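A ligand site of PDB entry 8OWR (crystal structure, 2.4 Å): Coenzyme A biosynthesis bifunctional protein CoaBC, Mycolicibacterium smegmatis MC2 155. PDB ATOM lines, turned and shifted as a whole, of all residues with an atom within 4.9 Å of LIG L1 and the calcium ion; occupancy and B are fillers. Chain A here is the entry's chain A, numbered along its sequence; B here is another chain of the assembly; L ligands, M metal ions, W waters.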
ATOM      1  N   MET A  98       1.596 -21.341 -20.869  1.00  0.00           N
ATOM      2  CA  MET A  98       1.141 -20.531 -22.004  1.00  0.00           C
ATOM      3  C   MET A  98       2.179 -19.448 -22.274  1.00  0.00           C
ATOM      4  O   MET A  98       1.991 -18.286 -21.946  1.00  0.00           O
ATOM      5  CB  MET A  98      -0.221 -19.918 -21.715  1.00  0.00           C
ATOM      6  CG  MET A  98      -1.474 -20.809 -21.835  1.00  0.00           C
ATOM      7  SD  MET A  98      -1.478 -22.017 -23.168  1.00  0.00           S
ATOM      8  CE  MET A  98      -2.070 -20.955 -24.472  1.00  0.00           C
ATOM      9  N   ALA A  99       3.293 -19.843 -22.912  1.00  0.00           N
ATOM     10  CA  ALA A  99       4.390 -18.902 -23.161  1.00  0.00           C
ATOM     11  C   ALA A  99       4.319 -18.229 -24.531  1.00  0.00           C
ATOM     12  O   ALA A  99       5.140 -17.367 -24.834  1.00  0.00           O
ATOM     13  CB  ALA A  99       5.748 -19.594 -22.992  1.00  0.00           C
ATOM     14  N   ALA A 100       3.375 -18.611 -25.371  1.00  0.00           N
ATOM     15  CA  ALA A 100       3.296 -18.054 -26.705  1.00  0.00           C
ATOM     16  C   ALA A 100       2.721 -16.637 -26.660  1.00  0.00           C
ATOM     17  O   ALA A 100       1.927 -16.281 -25.773  1.00  0.00           O
ATOM     18  CB  ALA A 100       2.441 -18.937 -27.599  1.00  0.00           C
ATOM     19  N   ALA A 101       3.169 -15.815 -27.602  1.00  0.00           N
ATOM     20  CA  ALA A 101       2.515 -14.533 -27.854  1.00  0.00           C
ATOM     21  C   ALA A 101       1.395 -14.792 -28.857  1.00  0.00           C
ATOM     22  O   ALA A 101       1.602 -14.726 -30.065  1.00  0.00           O
ATOM     23  CB  ALA A 101       3.498 -13.494 -28.358  1.00  0.00           C
ATOM     24  N   VAL A 102       0.201 -15.111 -28.351  1.00  0.00           N
ATOM     25  CA  VAL A 102      -0.944 -15.431 -29.197  1.00  0.00           C
ATOM     26  C   VAL A 102      -1.573 -14.140 -29.705  1.00  0.00           C
ATOM     27  O   VAL A 102      -1.901 -13.249 -28.929  1.00  0.00           O
ATOM     28  CB  VAL A 102      -1.985 -16.294 -28.448  1.00  0.00           C
ATOM     29  CG1 VAL A 102      -3.031 -16.830 -29.399  1.00  0.00           C
ATOM     30  CG2 VAL A 102      -1.331 -17.478 -27.716  1.00  0.00           C
ATOM     31  N   ALA A 103      -1.760 -14.056 -31.015  1.00  0.00           N
ATOM     32  CA  ALA A 103      -2.399 -12.906 -31.629  1.00  0.00           C
ATOM     33  C   ALA A 103      -3.833 -12.683 -31.123  1.00  0.00           C
ATOM     34  O   ALA A 103      -4.682 -13.572 -31.218  1.00  0.00           O
ATOM     35  CB  ALA A 103      -2.424 -13.094 -33.137  1.00  0.00           C
ATOM     36  N   ASP A 104      -4.112 -11.463 -30.659  1.00  0.00           N
ATOM     37  CA  ASP A 104      -5.474 -11.112 -30.242  1.00  0.00           C
ATOM     38  C   ASP A 104      -6.406 -10.927 -31.438  1.00  0.00           C
ATOM     39  O   ASP A 104      -7.626 -11.075 -31.287  1.00  0.00           O
ATOM     40  CB  ASP A 104      -5.473  -9.819 -29.420  1.00  0.00           C
ATOM     41  CG  ASP A 104      -4.907 -10.012 -28.027  1.00  0.00           C
ATOM     42  OD1 ASP A 104      -5.224 -11.034 -27.388  1.00  0.00           O
ATOM     43  OD2 ASP A 104      -4.113  -9.142 -27.607  1.00  0.00           O
ATOM     44  N   ASN A 130      -9.352 -13.179 -32.006  1.00  0.00           N
ATOM     45  CA  ASN A 130      -9.072 -14.593 -31.754  1.00  0.00           C
ATOM     46  C   ASN A 130      -9.453 -14.968 -30.327  1.00  0.00           C
ATOM     47  O   ASN A 130      -9.588 -14.120 -29.428  1.00  0.00           O
ATOM     48  CB  ASN A 130      -7.591 -14.921 -31.983  1.00  0.00           C
ATOM     49  CG  ASN A 130      -7.184 -14.899 -33.462  1.00  0.00           C
ATOM     50  OD1 ASN A 130      -7.928 -15.348 -34.341  1.00  0.00           O
ATOM     51  ND2 ASN A 130      -5.999 -14.358 -33.731  1.00  0.00           N
ATOM     52  N   ASP A 131      -9.669 -16.267 -30.124  1.00  0.00           N
ATOM     53  CA  ASP A 131      -9.977 -16.763 -28.796  1.00  0.00           C
ATOM     54  C   ASP A 131      -8.779 -16.609 -27.873  1.00  0.00           C
ATOM     55  O   ASP A 131      -7.622 -16.724 -28.309  1.00  0.00           O
ATOM     56  CB  ASP A 131     -10.418 -18.225 -28.853  1.00  0.00           C
ATOM     57  CG  ASP A 131     -11.733 -18.424 -29.567  1.00  0.00           C
ATOM     58  OD1 ASP A 131     -12.660 -17.597 -29.401  1.00  0.00           O
ATOM     59  OD2 ASP A 131     -11.838 -19.393 -30.338  1.00  0.00           O
ATOM     60  N   ASP A 132      -9.064 -16.308 -26.603  1.00  0.00           N
ATOM     61  CA  ASP A 132      -8.066 -16.299 -25.524  1.00  0.00           C
ATOM     62  C   ASP A 132      -7.913 -17.726 -25.051  1.00  0.00           C
ATOM     63  O   ASP A 132      -8.800 -18.266 -24.376  1.00  0.00           O
ATOM     64  CB  ASP A 132      -8.502 -15.333 -24.421  1.00  0.00           C
ATOM     65  CG  ASP A 132      -7.467 -15.182 -23.288  1.00  0.00           C
ATOM     66  OD1 ASP A 132      -6.506 -15.971 -23.172  1.00  0.00           O
ATOM     67  OD2 ASP A 132      -7.640 -14.214 -22.516  1.00  0.00           O
ATOM     68  N   VAL A 133      -6.826 -18.380 -25.465  1.00  0.00           N
ATOM     69  CA  VAL A 133      -6.640 -19.786 -25.143  1.00  0.00           C
ATOM     70  C   VAL A 133      -6.342 -19.962 -23.664  1.00  0.00           C
ATOM     71  O   VAL A 133      -6.847 -20.891 -23.027  1.00  0.00           O
ATOM     72  CB  VAL A 133      -5.550 -20.424 -26.032  1.00  0.00           C
ATOM     73  CG1 VAL A 133      -5.460 -21.927 -25.774  1.00  0.00           C
ATOM     74  CG2 VAL A 133      -5.812 -20.135 -27.535  1.00  0.00           C
ATOM     75  N   LEU A 134      -5.511 -19.076 -23.090  1.00  0.00           N
ATOM     76  CA  LEU A 134      -5.192 -19.220 -21.682  1.00  0.00           C
ATOM     77  C   LEU A 134      -6.450 -19.163 -20.822  1.00  0.00           C
ATOM     78  O   LEU A 134      -6.649 -19.992 -19.922  1.00  0.00           O
ATOM     79  CB  LEU A 134      -4.207 -18.139 -21.247  1.00  0.00           C
ATOM     80  CG  LEU A 134      -3.999 -18.114 -19.734  1.00  0.00           C
ATOM     81  CD1 LEU A 134      -3.479 -19.448 -19.257  1.00  0.00           C
ATOM     82  CD2 LEU A 134      -3.074 -16.945 -19.301  1.00  0.00           C
ATOM     83  N   GLY A 154       0.533 -18.537 -17.047  1.00  0.00           N
ATOM     84  CA  GLY A 154       0.509 -17.534 -18.094  1.00  0.00           C
ATOM     85  C   GLY A 154       1.765 -16.711 -18.157  1.00  0.00           C
ATOM     86  O   GLY A 154       2.556 -16.677 -17.200  1.00  0.00           O
ATOM     87  N   PHE A 155       1.992 -16.054 -19.283  1.00  0.00           N
ATOM     88  CA  PHE A 155       3.100 -15.125 -19.447  1.00  0.00           C
ATOM     89  C   PHE A 155       2.562 -13.739 -19.795  1.00  0.00           C
ATOM     90  O   PHE A 155       1.471 -13.600 -20.349  1.00  0.00           O
ATOM     91  CB  PHE A 155       4.073 -15.554 -20.543  1.00  0.00           C
ATOM     92  CG  PHE A 155       5.058 -16.573 -20.097  1.00  0.00           C
ATOM     93  CD1 PHE A 155       4.640 -17.814 -19.618  1.00  0.00           C
ATOM     94  CD2 PHE A 155       6.421 -16.303 -20.179  1.00  0.00           C
ATOM     95  CE1 PHE A 155       5.565 -18.762 -19.224  1.00  0.00           C
ATOM     96  CE2 PHE A 155       7.344 -17.255 -19.776  1.00  0.00           C
ATOM     97  CZ  PHE A 155       6.920 -18.486 -19.304  1.00  0.00           C
ATOM     98  N   ALA A 156       3.315 -12.710 -19.430  1.00  0.00           N
ATOM     99  CA  ALA A 156       2.942 -11.343 -19.789  1.00  0.00           C
ATOM    100  C   ALA A 156       4.212 -10.520 -19.960  1.00  0.00           C
ATOM    101  O   ALA A 156       5.142 -10.654 -19.159  1.00  0.00           O
ATOM    102  CB  ALA A 156       2.031 -10.681 -18.739  1.00  0.00           C
ATOM    103  N   ALA A 157       4.234  -9.677 -20.984  1.00  0.00           N
ATOM    104  CA  ALA A 157       5.262  -8.650 -21.104  1.00  0.00           C
ATOM    105  C   ALA A 157       4.582  -7.336 -20.765  1.00  0.00           C
ATOM    106  O   ALA A 157       3.780  -6.826 -21.554  1.00  0.00           O
ATOM    107  CB  ALA A 157       5.872  -8.615 -22.500  1.00  0.00           C
ATOM    108  N   GLU A 158       4.985  -6.729 -19.658  1.00  0.00           N
ATOM    109  CA  GLU A 158       4.272  -5.575 -19.129  1.00  0.00           C
ATOM    110  C   GLU A 158       5.190  -4.358 -19.048  1.00  0.00           C
ATOM    111  O   GLU A 158       6.421  -4.480 -19.051  1.00  0.00           O
ATOM    112  CB  GLU A 158       3.686  -5.870 -17.733  1.00  0.00           C
ATOM    113  CG  GLU A 158       2.479  -6.802 -17.691  1.00  0.00           C
ATOM    114  CD  GLU A 158       1.283  -6.310 -18.520  1.00  0.00           C
ATOM    115  OE1 GLU A 158       0.483  -7.166 -18.957  1.00  0.00           O
ATOM    116  OE2 GLU A 158       1.133  -5.083 -18.739  1.00  0.00           O
ATOM    117  N   LYS A 173      -3.360  -8.035 -14.602  1.00  0.00           N
ATOM    118  CA  LYS A 173      -3.411  -9.095 -15.603  1.00  0.00           C
ATOM    119  C   LYS A 173      -3.540 -10.455 -14.946  1.00  0.00           C
ATOM    120  O   LYS A 173      -4.318 -11.299 -15.387  1.00  0.00           O
ATOM    121  CB  LYS A 173      -2.179  -9.044 -16.506  1.00  0.00           C
ATOM    122  CG  LYS A 173      -2.368  -9.835 -17.790  1.00  0.00           C
ATOM    123  CD  LYS A 173      -2.387  -8.918 -19.016  1.00  0.00           C
ATOM    124  N   ARG A 176      -7.068 -10.839 -13.785  1.00  0.00           N
ATOM    125  CA  ARG A 176      -8.049 -10.979 -14.842  1.00  0.00           C
ATOM    126  C   ARG A 176      -7.984 -12.353 -15.495  1.00  0.00           C
ATOM    127  O   ARG A 176      -9.008 -12.942 -15.809  1.00  0.00           O
ATOM    128  CB  ARG A 176      -7.887  -9.818 -15.823  1.00  0.00           C
ATOM    129  CG  ARG A 176      -8.486 -10.031 -17.175  1.00  0.00           C
ATOM    130  CD  ARG A 176      -8.362  -8.754 -18.000  1.00  0.00           C
ATOM    131  NE  ARG A 176      -7.385  -7.794 -17.465  1.00  0.00           N
ATOM    132  CZ  ARG A 176      -6.263  -7.430 -18.092  1.00  0.00           C
ATOM    133  NH1 ARG A 176      -5.974  -7.939 -19.287  1.00  0.00           N
ATOM    134  NH2 ARG A 176      -5.444  -6.554 -17.534  1.00  0.00           N
ATOM    135  N   LYS A 177      -6.782 -12.894 -15.661  1.00  0.00           N
ATOM    136  CA  LYS A 177      -6.635 -14.188 -16.303  1.00  0.00           C
ATOM    137  C   LYS A 177      -7.019 -15.328 -15.382  1.00  0.00           C
ATOM    138  O   LYS A 177      -7.485 -16.374 -15.865  1.00  0.00           O
ATOM    139  CB  LYS A 177      -5.193 -14.345 -16.780  1.00  0.00           C
ATOM    140  CG  LYS A 177      -4.846 -13.272 -17.789  1.00  0.00           C
ATOM    141  CD  LYS A 177      -5.451 -13.593 -19.123  1.00  0.00           C
ATOM    142  CE  LYS A 177      -4.981 -12.612 -20.180  1.00  0.00           C
ATOM    143  NZ  LYS A 177      -5.376 -13.048 -21.562  1.00  0.00           N
ATOM    144  N   LYS B 116      -3.440  -2.417 -27.251  1.00  0.00           N
ATOM    145  CA  LYS B 116      -4.078  -3.311 -26.307  1.00  0.00           C
ATOM    146  C   LYS B 116      -5.362  -3.898 -26.879  1.00  0.00           C
ATOM    147  O   LYS B 116      -6.052  -3.279 -27.685  1.00  0.00           O
ATOM    148  CB  LYS B 116      -4.348  -2.591 -24.985  1.00  0.00           C
ATOM    149  CG  LYS B 116      -3.069  -2.290 -24.176  1.00  0.00           C
ATOM    150  CD  LYS B 116      -3.123  -2.875 -22.749  1.00  0.00           C
ATOM    151  CE  LYS B 116      -1.767  -2.785 -22.044  1.00  0.00           C
ATOM    152  NZ  LYS B 116      -1.702  -3.672 -20.843  1.00  0.00           N
ATOM    153  N   LYS B 117      -5.648  -5.148 -26.477  1.00  0.00           N
ATOM    154  CA  LYS B 117      -6.927  -5.791 -26.733  1.00  0.00           C
ATOM    155  C   LYS B 117      -7.934  -5.247 -25.734  1.00  0.00           C
ATOM    156  O   LYS B 117      -7.893  -5.595 -24.555  1.00  0.00           O
ATOM    157  CB  LYS B 117      -6.812  -7.305 -26.609  1.00  0.00           C
HETATM  158  N1  LIG L   1      -2.864 -15.833 -24.601  1.00  0.00           N
HETATM  159  C1  LIG L   1      -3.738 -16.809 -24.989  1.00  0.00           C
HETATM  160  N2  LIG L   1      -4.690 -16.495 -25.945  1.00  0.00           N
HETATM  161  C2  LIG L   1      -4.712 -15.235 -26.509  1.00  0.00           C
HETATM  162  C3  LIG L   1      -3.855 -14.268 -26.050  1.00  0.00           C
HETATM  163  C4  LIG L   1      -3.165 -14.544 -24.888  1.00  0.00           C
HETATM  164  O1  LIG L   1      -3.683 -17.930 -24.493  1.00  0.00           O
HETATM  165  N3  LIG L   1      -5.555 -14.943 -27.484  1.00  0.00           N
HETATM  166  C5  LIG L   1      -2.033 -16.084 -23.434  1.00  0.00           C
HETATM  167  C6  LIG L   1      -0.578 -15.746 -23.696  1.00  0.00           C
HETATM  168  O2  LIG L   1       0.152 -16.850 -24.158  1.00  0.00           O
HETATM  169  C7  LIG L   1      -0.126 -15.304 -22.315  1.00  0.00           C
HETATM  170  C8  LIG L   1      -1.371 -14.777 -21.634  1.00  0.00           C
HETATM  171  O3  LIG L   1      -2.448 -15.191 -22.426  1.00  0.00           O
HETATM  172  O4  LIG L   1       0.239 -16.394 -21.520  1.00  0.00           O
HETATM  173  C9  LIG L   1      -1.431 -13.269 -21.460  1.00  0.00           C
HETATM  174  O5  LIG L   1      -0.898 -12.609 -22.583  1.00  0.00           O
HETATM  175  P1  LIG L   1      -1.190 -11.031 -22.732  1.00  0.00           P
HETATM  176  O6  LIG L   1      -0.976 -10.692 -24.182  1.00  0.00           O
HETATM  177  O7  LIG L   1      -0.299 -10.221 -21.822  1.00  0.00           O
HETATM  178  O8  LIG L   1      -2.738 -10.888 -22.262  1.00  0.00           O
HETATM  179  P2  LIG L   1      -3.771  -9.860 -22.940  1.00  0.00           P
HETATM  180  O9  LIG L   1      -5.169 -10.006 -22.392  1.00  0.00           O
HETATM  181  O10 LIG L   1      -3.796 -10.070 -24.435  1.00  0.00           O
HETATM  182  O11 LIG L   1      -3.124  -8.465 -22.462  1.00  0.00           O
HETATM  183  P3  LIG L   1      -3.082  -7.116 -23.330  1.00  0.00           P
HETATM  184  O12 LIG L   1      -4.461  -6.934 -23.919  1.00  0.00           O
HETATM  185  O13 LIG L   1      -2.648  -5.956 -22.451  1.00  0.00           O
HETATM  186  O14 LIG L   1      -2.120  -7.259 -24.468  1.00  0.00           O
HETATM  187  C1  LG2 L   2       4.741 -12.608 -24.550  1.00  0.00           C
HETATM  188  C2  LG2 L   2       2.438 -11.122 -24.952  1.00  0.00           C
HETATM  189  C3  LG2 L   2       4.777 -11.422 -25.271  1.00  0.00           C
HETATM  190  C4  LG2 L   2       9.349 -14.182 -18.870  1.00  0.00           C
HETATM  191  C5  LG2 L   2      11.619 -13.820 -18.198  1.00  0.00           C
HETATM  192  C6  LG2 L   2      10.930 -13.244 -20.413  1.00  0.00           C
HETATM  193  C7  LG2 L   2       8.893 -14.062 -22.526  1.00  0.00           C
HETATM  194  C8  LG2 L   2       8.607 -13.558 -21.245  1.00  0.00           C
HETATM  195  C9  LG2 L   2       7.406 -12.895 -21.004  1.00  0.00           C
HETATM  196  C10 LG2 L   2       6.475 -12.744 -22.028  1.00  0.00           C
HETATM  197  C11 LG2 L   2       6.761 -13.265 -23.306  1.00  0.00           C
HETATM  198  C12 LG2 L   2       7.956 -13.914 -23.563  1.00  0.00           C
HETATM  199  C13 LG2 L   2       7.912 -14.283 -24.922  1.00  0.00           C
HETATM  200  C14 LG2 L   2       6.688 -13.833 -25.400  1.00  0.00           C
HETATM  201  C15 LG2 L   2       3.555 -13.055 -24.010  1.00  0.00           C
HETATM  202  C16 LG2 L   2       2.401 -12.312 -24.223  1.00  0.00           C
HETATM  203  C17 LG2 L   2       3.636 -10.665 -25.475  1.00  0.00           C
HETATM  204  C18 LG2 L   2       8.968 -15.047 -25.737  1.00  0.00           C
HETATM  205  C19 LG2 L   2       9.979 -15.921 -25.028  1.00  0.00           C
HETATM  206  C20 LG2 L   2       9.640 -13.694 -20.127  1.00  0.00           C
HETATM  207  C21 LG2 L   2      10.342 -14.256 -17.904  1.00  0.00           C
HETATM  208  C22 LG2 L   2      11.924 -13.302 -19.451  1.00  0.00           C
HETATM  209  N1  LG2 L   2       6.031 -13.256 -24.424  1.00  0.00           N
HETATM  210  O1  LG2 L   2       3.694  -9.468 -26.200  1.00  0.00           O
HETATM  211  O2  LG2 L   2       1.298 -10.361 -25.166  1.00  0.00           O
HETATM  212  O3  LG2 L   2      11.110 -15.449 -24.742  1.00  0.00           O
HETATM  213  O4  LG2 L   2       9.676 -17.095 -24.737  1.00  0.00           O
HETATM  214  O5  LG2 L   2       9.023 -14.982 -26.918  1.00  0.00           O
HETATM  215  O6  LG2 L   2      13.217 -12.857 -19.761  1.00  0.00           O
HETATM  216 CA    CA M   1      -1.992  -9.424 -25.970  1.00  0.00          CA
HETATM  217  O   HOH W   1      -6.409 -12.364 -24.579  1.00  0.00           O
HETATM  218  O   HOH W   2       1.920  -9.115 -22.302  1.00  0.00           O
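N of Val 133 lies within hydrogen-bond range of N2 of LIG L1 (2.9 Å). NZ of Lys 177 lies within salt-bridge range of O9 of LIG L1 (3.2 Å). An oxygen (O4) of LIG L1 lies within hydrogen-bond range of the backbone carbonyl oxygen (O) of Met 98 (2.6 Å). N of Phe 155 is in hydrogen-bond range of O4 of LIG L1 (2.9 Å). NZ of Lys 116 of chain B is in salt-bridge range of O13 of LIG L1, 2.9 Å away. N of Leu 134 sits at hydrogen-bond distance from O1 of LIG L1. NH1 of Arg 176 lies within salt-bridge range of O9 of LIG L1 (3.8 Å). A nitrogen (N3) of LIG L1 lies within hydrogen-bond range of the backbone carbonyl oxygen (O) of Asp 131, at 2.9 Å. O of Ala 100 is in hydrogen-bond range of O2 of LIG L1 (2.5 Å). The backbone NH of Lys 117 of chain B is in hydrogen-bond range of an oxygen (O12) of LIG L1 (3.3 Å). O of Phe 155 sits close to O4 of LIG L1.
An oxygen (O6) of LIG L1 sits close to an oxygen (O2) of LG2 L2 (2.5 Å).
The backbone NH (N) of Leu 134 is in hydrogen-bond range of the side-chain carboxylate (OD1) of Asp 132, 3.3 Å away. The side-chain carboxylate of Glu 158 lies within salt-bridge range of the side-chain amino group of Lys 116 of chain B. The backbone carbonyl oxygen of Met 98 is in hydrogen-bond range of the backbone NH of Phe 155 (3.5 Å). O of Asp 104 is in hydrogen-bond range of N of Asn 130, at 2.8 Å. The side-chain amino group (NZ) of Lys 177 lies within salt-bridge range of the side-chain carboxylate (OD2) of Asp 132 (2.7 Å).
OD1 of Asp 132 lies close to N2 of LIG L1 (3.4 Å). CB of Val 102 touches C2 of LIG L1, 3.5 Å away. Gly 154 touches LIG L1 (CA to O4, 3.6 Å). CB of Ala 156 touches O7 of LIG L1, 3.9 Å away. Lys 173 touches LIG L1. Hydrophobic or aromatic side chains within 4 Å of LIG L1: Met 98, Val 102, Val 133, Leu 134 and Ala 156. Of the 22 residues printed, 16 come within 4 Å of LIG L1.
The nearest printed residue that does not touch the calcium ion is Val 102 (4.8 Å).
The calcium ion is bound by an oxygen (O6) of LIG L1, an oxygen (O10) of LIG L1, an oxygen (O14) of LIG L1 and the side-chain carboxylate of Asp 104.
Water W2 lies within hydrogen-bond range of O7 of LIG L1 (2.5 Å), N of Ala 157 (2.7 Å) and O2 of LG2 L2 (3.2 Å). Water W1 lies within hydrogen-bond range of OD2 of Asp 132, NZ of Lys 177, OD1 of Asp 104 and O9 of LIG L1.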
